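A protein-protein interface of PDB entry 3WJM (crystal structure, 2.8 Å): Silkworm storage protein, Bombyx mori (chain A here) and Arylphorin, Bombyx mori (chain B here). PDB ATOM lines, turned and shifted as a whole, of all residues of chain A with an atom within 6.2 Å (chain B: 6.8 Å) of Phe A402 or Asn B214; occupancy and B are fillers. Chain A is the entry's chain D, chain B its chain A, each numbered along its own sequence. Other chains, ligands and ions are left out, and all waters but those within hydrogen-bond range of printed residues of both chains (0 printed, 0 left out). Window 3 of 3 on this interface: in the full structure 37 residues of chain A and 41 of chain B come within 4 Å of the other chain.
The backbone carbonyl oxygen (O) of Val B216 sits at hydrogen-bond distance from the side-chain hydroxyl (OH) of Tyr A307.
The side-chain hydroxyl (OG1) of Thr B226 sits at hydrogen-bond distance from the side-chain amide oxygen (OD1) of Asn B214, at 3.3 Å. The side-chain amide nitrogen of Gln B223 lies within hydrogen-bond range of the backbone carbonyl oxygen of Leu B217.
Among the printed residues, merely in contact across the chains: Phe A402 with Ala B215 (3.2 Å), Phe A402 with Val B216 (3.5 Å), Phe A402 with Leu B217 (3.6 Å), Tyr A307 with Leu B304 (3.9 Å) and Phe A402 with Asn B214 (3.9 Å).
Printed residues of chain B within 4 Å of Tyr A307: Val B216 (2.6 Å) and Leu B304 (3.9 Å). Asn A403 touches none of the printed residues of chain B. Of the printed residues of chain A, Asn B214 touches Phe A402 (3.9 Å). Of the printed residues of chain A, Ala B215 touches Phe A402. Printed residues of chain A within 4 Å of Val B216: Tyr A307 and Phe A402. Of the printed residues of chain A, Leu B217 touches Phe A402 (3.6 Å). Glu B230 touches none of the printed residues of chain A. Of the printed residues of chain A, Leu B304 touches Tyr A307. The nearest residue of chain B that does not touch Phe A402 is Tyr B218 (4.3 Å).
Hydrophobic or aromatic side chains of chain A within 4 Å of the printed part of chain B: Tyr A307 and Phe A402. Hydrophobic or aromatic side chains of chain B within 4 Å of the printed part of chain A: Val B216 and Leu B304. Among the printed residues, 6 pairs touch across the chains. Among the printed residues, no Asp or Glu carboxylate lies within 4 Å of a Lys or Arg side-chain nitrogen of the other chain.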
ATOM      1  N   TYR A 307      30.335  18.063  20.245  1.00  0.00           N
ATOM      2  CA  TYR A 307      29.639  17.696  21.457  1.00  0.00           C
ATOM      3  C   TYR A 307      30.620  17.359  22.539  1.00  0.00           C
ATOM      4  O   TYR A 307      31.603  16.684  22.291  1.00  0.00           O
ATOM      5  CB  TYR A 307      28.789  16.444  21.246  1.00  0.00           C
ATOM      6  CG  TYR A 307      27.882  16.441  20.030  1.00  0.00           C
ATOM      7  CD1 TYR A 307      28.167  15.630  18.917  1.00  0.00           C
ATOM      8  CD2 TYR A 307      26.709  17.195  20.011  1.00  0.00           C
ATOM      9  CE1 TYR A 307      27.317  15.599  17.802  1.00  0.00           C
ATOM     10  CE2 TYR A 307      25.856  17.165  18.910  1.00  0.00           C
ATOM     11  CZ  TYR A 307      26.161  16.379  17.810  1.00  0.00           C
ATOM     12  OH  TYR A 307      25.309  16.392  16.721  1.00  0.00           O
ATOM     13  N   PRO A 399      22.184  11.239  23.904  1.00  0.00           N
ATOM     14  CA  PRO A 399      21.006  11.539  23.045  1.00  0.00           C
ATOM     15  C   PRO A 399      21.042  10.811  21.705  1.00  0.00           C
ATOM     16  O   PRO A 399      22.097  10.423  21.226  1.00  0.00           O
ATOM     17  CB  PRO A 399      21.113  13.042  22.792  1.00  0.00           C
ATOM     18  CG  PRO A 399      21.958  13.568  23.904  1.00  0.00           C
ATOM     19  CD  PRO A 399      22.823  12.453  24.432  1.00  0.00           C
ATOM     20  N   LYS A 400      19.896  10.632  21.086  1.00  0.00           N
ATOM     21  CA  LYS A 400      19.861   9.820  19.881  1.00  0.00           C
ATOM     22  C   LYS A 400      20.509  10.560  18.709  1.00  0.00           C
ATOM     23  O   LYS A 400      20.485  11.796  18.687  1.00  0.00           O
ATOM     24  CB  LYS A 400      18.438   9.321  19.632  1.00  0.00           C
ATOM     25  CG  LYS A 400      17.947   8.501  20.839  1.00  0.00           C
ATOM     26  CD  LYS A 400      17.033   7.351  20.423  1.00  0.00           C
ATOM     27  CE  LYS A 400      17.531   5.993  20.925  1.00  0.00           C
ATOM     28  NZ  LYS A 400      17.011   4.900  20.039  1.00  0.00           N
ATOM     29  N   PRO A 401      21.141   9.814  17.761  1.00  0.00           N
ATOM     30  CA  PRO A 401      22.008  10.492  16.793  1.00  0.00           C
ATOM     31  C   PRO A 401      21.287  11.552  15.979  1.00  0.00           C
ATOM     32  O   PRO A 401      20.105  11.418  15.687  1.00  0.00           O
ATOM     33  CB  PRO A 401      22.508   9.352  15.896  1.00  0.00           C
ATOM     34  CG  PRO A 401      22.350   8.121  16.725  1.00  0.00           C
ATOM     35  CD  PRO A 401      21.121   8.357  17.533  1.00  0.00           C
ATOM     36  N   PHE A 402      22.013  12.596  15.608  1.00  0.00           N
ATOM     37  CA  PHE A 402      21.436  13.687  14.863  1.00  0.00           C
ATOM     38  C   PHE A 402      21.160  13.311  13.400  1.00  0.00           C
ATOM     39  O   PHE A 402      20.189  13.755  12.816  1.00  0.00           O
ATOM     40  CB  PHE A 402      22.354  14.906  14.971  1.00  0.00           C
ATOM     41  CG  PHE A 402      21.831  16.120  14.268  1.00  0.00           C
ATOM     42  CD1 PHE A 402      22.396  16.532  13.058  1.00  0.00           C
ATOM     43  CD2 PHE A 402      20.768  16.843  14.806  1.00  0.00           C
ATOM     44  CE1 PHE A 402      21.915  17.658  12.405  1.00  0.00           C
ATOM     45  CE2 PHE A 402      20.285  17.974  14.163  1.00  0.00           C
ATOM     46  CZ  PHE A 402      20.858  18.379  12.959  1.00  0.00           C
ATOM     47  N   ASN A 403      22.044  12.511  12.814  1.00  0.00           N
ATOM     48  CA  ASN A 403      21.836  11.912  11.485  1.00  0.00           C
ATOM     49  C   ASN A 403      22.796  10.756  11.424  1.00  0.00           C
ATOM     50  O   ASN A 403      23.472  10.496  12.420  1.00  0.00           O
ATOM     51  CB  ASN A 403      22.010  12.919  10.318  1.00  0.00           C
ATOM     52  CG  ASN A 403      23.472  13.319  10.041  1.00  0.00           C
ATOM     53  OD1 ASN A 403      24.440  12.726  10.554  1.00  0.00           O
ATOM     54  ND2 ASN A 403      23.634  14.328   9.189  1.00  0.00           N
ATOM     55  N   GLN A 404      22.894  10.084  10.281  1.00  0.00           N
ATOM     56  CA  GLN A 404      23.627   8.830  10.270  1.00  0.00           C
ATOM     57  C   GLN A 404      25.130   8.988  10.363  1.00  0.00           C
ATOM     58  O   GLN A 404      25.852   8.020  10.587  1.00  0.00           O
ATOM     59  CB  GLN A 404      23.181   7.914   9.127  1.00  0.00           C
ATOM     60  CG  GLN A 404      21.982   7.059   9.549  1.00  0.00           C
ATOM     61  CD  GLN A 404      21.617   5.976   8.556  1.00  0.00           C
ATOM     62  OE1 GLN A 404      21.112   6.270   7.479  1.00  0.00           O
ATOM     63  NE2 GLN A 404      21.881   4.711   8.911  1.00  0.00           N
ATOM     64  N   THR A 406      26.457  11.566  12.327  1.00  0.00           N
ATOM     65  CA  THR A 406      26.704  12.441  13.460  1.00  0.00           C
ATOM     66  C   THR A 406      26.004  11.849  14.639  1.00  0.00           C
ATOM     67  O   THR A 406      24.763  11.951  14.749  1.00  0.00           O
ATOM     68  CB  THR A 406      26.108  13.844  13.244  1.00  0.00           C
ATOM     69  OG1 THR A 406      26.273  14.226  11.883  1.00  0.00           O
ATOM     70  CG2 THR A 406      26.773  14.889  14.129  1.00  0.00           C
ATOM     71  N   PHE A 407      26.778  11.229  15.519  1.00  0.00           N
ATOM     72  CA  PHE A 407      26.243  10.783  16.788  1.00  0.00           C
ATOM     73  C   PHE A 407      26.815  11.613  17.943  1.00  0.00           C
ATOM     74  O   PHE A 407      27.782  12.349  17.758  1.00  0.00           O
ATOM     75  CB  PHE A 407      26.480   9.269  16.970  1.00  0.00           C
ATOM     76  CG  PHE A 407      27.927   8.859  17.001  1.00  0.00           C
ATOM     77  CD1 PHE A 407      28.647   8.705  15.829  1.00  0.00           C
ATOM     78  CD2 PHE A 407      28.562   8.572  18.225  1.00  0.00           C
ATOM     79  CE1 PHE A 407      29.984   8.313  15.870  1.00  0.00           C
ATOM     80  CE2 PHE A 407      29.879   8.157  18.270  1.00  0.00           C
ATOM     81  CZ  PHE A 407      30.592   8.053  17.089  1.00  0.00           C
ATOM     82  N   ILE A 408      26.222  11.507  19.127  1.00  0.00           N
ATOM     83  CA  ILE A 408      26.768  12.162  20.288  1.00  0.00           C
ATOM     84  C   ILE A 408      27.617  11.163  21.054  1.00  0.00           C
ATOM     85  O   ILE A 408      27.125  10.183  21.535  1.00  0.00           O
ATOM     86  CB  ILE A 408      25.678  12.753  21.156  1.00  0.00           C
ATOM     87  CG1 ILE A 408      25.045  13.930  20.412  1.00  0.00           C
ATOM     88  CG2 ILE A 408      26.293  13.286  22.429  1.00  0.00           C
ATOM     89  CD1 ILE A 408      23.744  13.663  19.694  1.00  0.00           C
ATOM     90  N   ASN B 172      28.735  27.902  21.335  1.00  0.00           N
ATOM     91  CA  ASN B 172      29.013  26.464  21.433  1.00  0.00           C
ATOM     92  C   ASN B 172      30.453  26.103  21.064  1.00  0.00           C
ATOM     93  O   ASN B 172      31.224  26.930  20.576  1.00  0.00           O
ATOM     94  CB  ASN B 172      28.005  25.677  20.611  1.00  0.00           C
ATOM     95  CG  ASN B 172      26.604  26.248  20.725  1.00  0.00           C
ATOM     96  OD1 ASN B 172      26.153  26.609  21.800  1.00  0.00           O
ATOM     97  ND2 ASN B 172      25.928  26.380  19.594  1.00  0.00           N
ATOM     98  N   ASN B 211      25.990  28.683  14.137  1.00  0.00           N
ATOM     99  CA  ASN B 211      24.594  28.320  14.291  1.00  0.00           C
ATOM    100  C   ASN B 211      24.190  28.259  15.776  1.00  0.00           C
ATOM    101  O   ASN B 211      25.017  28.220  16.698  1.00  0.00           O
ATOM    102  CB  ASN B 211      24.346  26.950  13.703  1.00  0.00           C
ATOM    103  CG  ASN B 211      24.335  26.927  12.198  1.00  0.00           C
ATOM    104  OD1 ASN B 211      23.893  27.850  11.514  1.00  0.00           O
ATOM    105  ND2 ASN B 211      24.821  25.840  11.668  1.00  0.00           N
ATOM    106  N   TYR B 212      22.886  28.217  15.998  1.00  0.00           N
ATOM    107  CA  TYR B 212      22.348  27.958  17.313  1.00  0.00           C
ATOM    108  C   TYR B 212      22.439  26.450  17.518  1.00  0.00           C
ATOM    109  O   TYR B 212      22.709  25.730  16.581  1.00  0.00           O
ATOM    110  CB  TYR B 212      20.945  28.509  17.358  1.00  0.00           C
ATOM    111  CG  TYR B 212      20.982  30.014  17.355  1.00  0.00           C
ATOM    112  CD1 TYR B 212      21.516  30.701  18.442  1.00  0.00           C
ATOM    113  CD2 TYR B 212      20.484  30.764  16.296  1.00  0.00           C
ATOM    114  CE1 TYR B 212      21.552  32.082  18.481  1.00  0.00           C
ATOM    115  CE2 TYR B 212      20.507  32.158  16.330  1.00  0.00           C
ATOM    116  CZ  TYR B 212      21.058  32.806  17.430  1.00  0.00           C
ATOM    117  OH  TYR B 212      21.133  34.181  17.530  1.00  0.00           O
ATOM    118  N   SER B 213      22.263  25.955  18.731  1.00  0.00           N
ATOM    119  CA  SER B 213      22.598  24.561  18.985  1.00  0.00           C
ATOM    120  C   SER B 213      21.653  23.589  18.287  1.00  0.00           C
ATOM    121  O   SER B 213      22.002  22.409  18.108  1.00  0.00           O
ATOM    122  CB  SER B 213      22.602  24.272  20.465  1.00  0.00           C
ATOM    123  OG  SER B 213      21.261  24.294  20.953  1.00  0.00           O
ATOM    124  N   ASN B 214      20.463  24.045  17.888  1.00  0.00           N
ATOM    125  CA  ASN B 214      19.529  23.076  17.296  1.00  0.00           C
ATOM    126  C   ASN B 214      20.019  22.531  15.957  1.00  0.00           C
ATOM    127  O   ASN B 214      19.503  21.547  15.476  1.00  0.00           O
ATOM    128  CB  ASN B 214      18.162  23.685  17.106  1.00  0.00           C
ATOM    129  CG  ASN B 214      18.233  24.921  16.296  1.00  0.00           C
ATOM    130  OD1 ASN B 214      18.671  25.958  16.807  1.00  0.00           O
ATOM    131  ND2 ASN B 214      17.887  24.827  15.012  1.00  0.00           N
ATOM    132  N   ALA B 215      20.990  23.212  15.349  1.00  0.00           N
ATOM    133  CA  ALA B 215      21.628  22.776  14.116  1.00  0.00           C
ATOM    134  C   ALA B 215      22.471  21.463  14.262  1.00  0.00           C
ATOM    135  O   ALA B 215      22.839  20.854  13.270  1.00  0.00           O
ATOM    136  CB  ALA B 215      22.468  23.904  13.559  1.00  0.00           C
ATOM    137  N   VAL B 216      22.767  21.034  15.489  1.00  0.00           N
ATOM    138  CA  VAL B 216      23.450  19.769  15.706  1.00  0.00           C
ATOM    139  C   VAL B 216      22.716  18.944  16.776  1.00  0.00           C
ATOM    140  O   VAL B 216      23.190  17.897  17.172  1.00  0.00           O
ATOM    141  CB  VAL B 216      24.953  19.960  16.118  1.00  0.00           C
ATOM    142  CG1 VAL B 216      25.775  20.607  14.998  1.00  0.00           C
ATOM    143  CG2 VAL B 216      25.091  20.727  17.443  1.00  0.00           C
ATOM    144  N   LEU B 217      21.564  19.406  17.237  1.00  0.00           N
ATOM    145  CA  LEU B 217      20.952  18.834  18.438  1.00  0.00           C
ATOM    146  C   LEU B 217      19.480  19.171  18.475  1.00  0.00           C
ATOM    147  O   LEU B 217      19.131  20.329  18.685  1.00  0.00           O
ATOM    148  CB  LEU B 217      21.615  19.400  19.715  1.00  0.00           C
ATOM    149  CG  LEU B 217      21.451  18.582  21.011  1.00  0.00           C
ATOM    150  CD1 LEU B 217      22.167  17.246  20.912  1.00  0.00           C
ATOM    151  CD2 LEU B 217      21.875  19.303  22.291  1.00  0.00           C
ATOM    152  N   TYR B 218      18.624  18.176  18.251  1.00  0.00           N
ATOM    153  CA  TYR B 218      17.188  18.335  18.452  1.00  0.00           C
ATOM    154  C   TYR B 218      16.698  17.231  19.404  1.00  0.00           C
ATOM    155  O   TYR B 218      15.973  16.310  19.043  1.00  0.00           O
ATOM    156  CB  TYR B 218      16.408  18.425  17.125  1.00  0.00           C
ATOM    157  CG  TYR B 218      14.977  18.939  17.277  1.00  0.00           C
ATOM    158  CD1 TYR B 218      14.703  20.313  17.457  1.00  0.00           C
ATOM    159  CD2 TYR B 218      13.890  18.050  17.244  1.00  0.00           C
ATOM    160  CE1 TYR B 218      13.398  20.785  17.603  1.00  0.00           C
ATOM    161  CE2 TYR B 218      12.577  18.504  17.394  1.00  0.00           C
ATOM    162  CZ  TYR B 218      12.320  19.875  17.577  1.00  0.00           C
ATOM    163  OH  TYR B 218      10.985  20.310  17.718  1.00  0.00           O
ATOM    164  N   GLN B 223      13.999  22.962  21.733  1.00  0.00           N
ATOM    165  CA  GLN B 223      15.042  23.478  20.829  1.00  0.00           C
ATOM    166  C   GLN B 223      14.495  24.435  19.770  1.00  0.00           C
ATOM    167  O   GLN B 223      15.264  25.087  19.045  1.00  0.00           O
ATOM    168  CB  GLN B 223      15.843  22.358  20.143  1.00  0.00           C
ATOM    169  CG  GLN B 223      16.710  21.509  21.068  1.00  0.00           C
ATOM    170  CD  GLN B 223      17.936  22.249  21.568  1.00  0.00           C
ATOM    171  OE1 GLN B 223      17.903  22.939  22.597  1.00  0.00           O
ATOM    172  NE2 GLN B 223      19.040  22.081  20.862  1.00  0.00           N
ATOM    173  N   ARG B 224      13.176  24.526  19.666  1.00  0.00           N
ATOM    174  CA  ARG B 224      12.596  25.487  18.766  1.00  0.00           C
ATOM    175  C   ARG B 224      13.006  26.916  19.154  1.00  0.00           C
ATOM    176  O   ARG B 224      13.098  27.783  18.303  1.00  0.00           O
ATOM    177  CB  ARG B 224      11.068  25.339  18.711  1.00  0.00           C
ATOM    178  CG  ARG B 224      10.561  24.085  17.968  1.00  0.00           C
ATOM    179  CD  ARG B 224       9.049  23.933  18.056  1.00  0.00           C
ATOM    180  NE  ARG B 224       8.610  22.545  17.891  1.00  0.00           N
ATOM    181  CZ  ARG B 224       7.334  22.135  17.894  1.00  0.00           C
ATOM    182  NH1 ARG B 224       6.334  22.988  18.055  1.00  0.00           N
ATOM    183  NH2 ARG B 224       7.042  20.848  17.744  1.00  0.00           N
ATOM    184  N   LEU B 225      13.311  27.151  20.425  1.00  0.00           N
ATOM    185  CA  LEU B 225      13.423  28.511  20.944  1.00  0.00           C
ATOM    186  C   LEU B 225      14.853  29.084  21.040  1.00  0.00           C
ATOM    187  O   LEU B 225      15.084  30.161  21.617  1.00  0.00           O
ATOM    188  CB  LEU B 225      12.703  28.581  22.305  1.00  0.00           C
ATOM    189  CG  LEU B 225      11.297  27.966  22.316  1.00  0.00           C
ATOM    190  CD1 LEU B 225      10.802  27.883  23.729  1.00  0.00           C
ATOM    191  CD2 LEU B 225      10.332  28.816  21.501  1.00  0.00           C
ATOM    192  N   THR B 226      15.800  28.371  20.459  1.00  0.00           N
ATOM    193  CA  THR B 226      17.215  28.712  20.507  1.00  0.00           C
ATOM    194  C   THR B 226      17.638  30.120  20.064  1.00  0.00           C
ATOM    195  O   THR B 226      18.540  30.687  20.641  1.00  0.00           O
ATOM    196  CB  THR B 226      17.987  27.777  19.588  1.00  0.00           C
ATOM    197  OG1 THR B 226      17.580  26.457  19.830  1.00  0.00           O
ATOM    198  CG2 THR B 226      19.422  27.835  19.893  1.00  0.00           C
ATOM    199  N   TYR B 227      17.056  30.640  18.999  1.00  0.00           N
ATOM    200  CA  TYR B 227      17.424  31.966  18.536  1.00  0.00           C
ATOM    201  C   TYR B 227      17.032  32.994  19.588  1.00  0.00           C
ATOM    202  O   TYR B 227      17.467  34.140  19.521  1.00  0.00           O
ATOM    203  CB  TYR B 227      16.730  32.316  17.206  1.00  0.00           C
ATOM    204  CG  TYR B 227      15.230  32.327  17.360  1.00  0.00           C
ATOM    205  CD1 TYR B 227      14.479  31.177  17.083  1.00  0.00           C
ATOM    206  CD2 TYR B 227      14.568  33.453  17.866  1.00  0.00           C
ATOM    207  CE1 TYR B 227      13.102  31.167  17.242  1.00  0.00           C
ATOM    208  CE2 TYR B 227      13.185  33.445  18.049  1.00  0.00           C
ATOM    209  CZ  TYR B 227      12.455  32.302  17.727  1.00  0.00           C
ATOM    210  OH  TYR B 227      11.091  32.273  17.908  1.00  0.00           O
ATOM    211  N   GLU B 230      19.284  31.300  23.346  1.00  0.00           N
ATOM    212  CA  GLU B 230      20.733  31.416  23.099  1.00  0.00           C
ATOM    213  C   GLU B 230      21.157  32.795  22.606  1.00  0.00           C
ATOM    214  O   GLU B 230      22.350  33.064  22.507  1.00  0.00           O
ATOM    215  CB  GLU B 230      21.242  30.331  22.121  1.00  0.00           C
ATOM    216  CG  GLU B 230      21.509  28.962  22.760  1.00  0.00           C
ATOM    217  CD  GLU B 230      21.915  27.856  21.756  1.00  0.00           C
ATOM    218  OE1 GLU B 230      22.634  28.102  20.733  1.00  0.00           O
ATOM    219  OE2 GLU B 230      21.488  26.709  21.998  1.00  0.00           O
ATOM    220  N   LEU B 304      26.447  22.595  25.073  1.00  0.00           N
ATOM    221  CA  LEU B 304      27.617  22.438  24.200  1.00  0.00           C
ATOM    222  C   LEU B 304      28.682  23.504  24.483  1.00  0.00           C
ATOM    223  O   LEU B 304      29.487  23.788  23.628  1.00  0.00           O
ATOM    224  CB  LEU B 304      27.227  22.480  22.713  1.00  0.00           C
ATOM    225  CG  LEU B 304      25.986  21.732  22.225  1.00  0.00           C
ATOM    226  CD1 LEU B 304      25.632  22.123  20.807  1.00  0.00           C
ATOM    227  CD2 LEU B 304      26.137  20.237  22.329  1.00  0.00           C
ATOM    228  N   PRO B 685      17.286  30.331  11.174  1.00  0.00           N
ATOM    229  CA  PRO B 685      18.600  30.967  11.167  1.00  0.00           C
ATOM    230  C   PRO B 685      19.700  30.195  10.443  1.00  0.00           C
ATOM    231  O   PRO B 685      20.494  30.786   9.768  1.00  0.00           O
ATOM    232  CB  PRO B 685      18.903  31.113  12.644  1.00  0.00           C
ATOM    233  CG  PRO B 685      17.554  31.342  13.212  1.00  0.00           C
ATOM    234  CD  PRO B 685      16.695  30.341  12.520  1.00  0.00           C
ATOM    235  N   TYR B 686      19.752  28.887  10.562  1.00  0.00           N
ATOM    236  CA  TYR B 686      20.825  28.153   9.932  1.00  0.00           C
ATOM    237  C   TYR B 686      20.891  28.409   8.424  1.00  0.00           C
ATOM    238  O   TYR B 686      21.948  28.220   7.814  1.00  0.00           O
ATOM    239  CB  TYR B 686      20.674  26.672  10.225  1.00  0.00           C
ATOM    240  CG  TYR B 686      19.635  25.949   9.389  1.00  0.00           C
ATOM    241  CD1 TYR B 686      18.453  25.472   9.970  1.00  0.00           C
ATOM    242  CD2 TYR B 686      19.850  25.712   8.013  1.00  0.00           C
ATOM    243  CE1 TYR B 686      17.515  24.792   9.209  1.00  0.00           C
ATOM    244  CE2 TYR B 686      18.930  25.027   7.247  1.00  0.00           C
ATOM    245  CZ  TYR B 686      17.778  24.578   7.852  1.00  0.00           C
ATOM    246  OH  TYR B 686      16.869  23.937   7.088  1.00  0.00           O
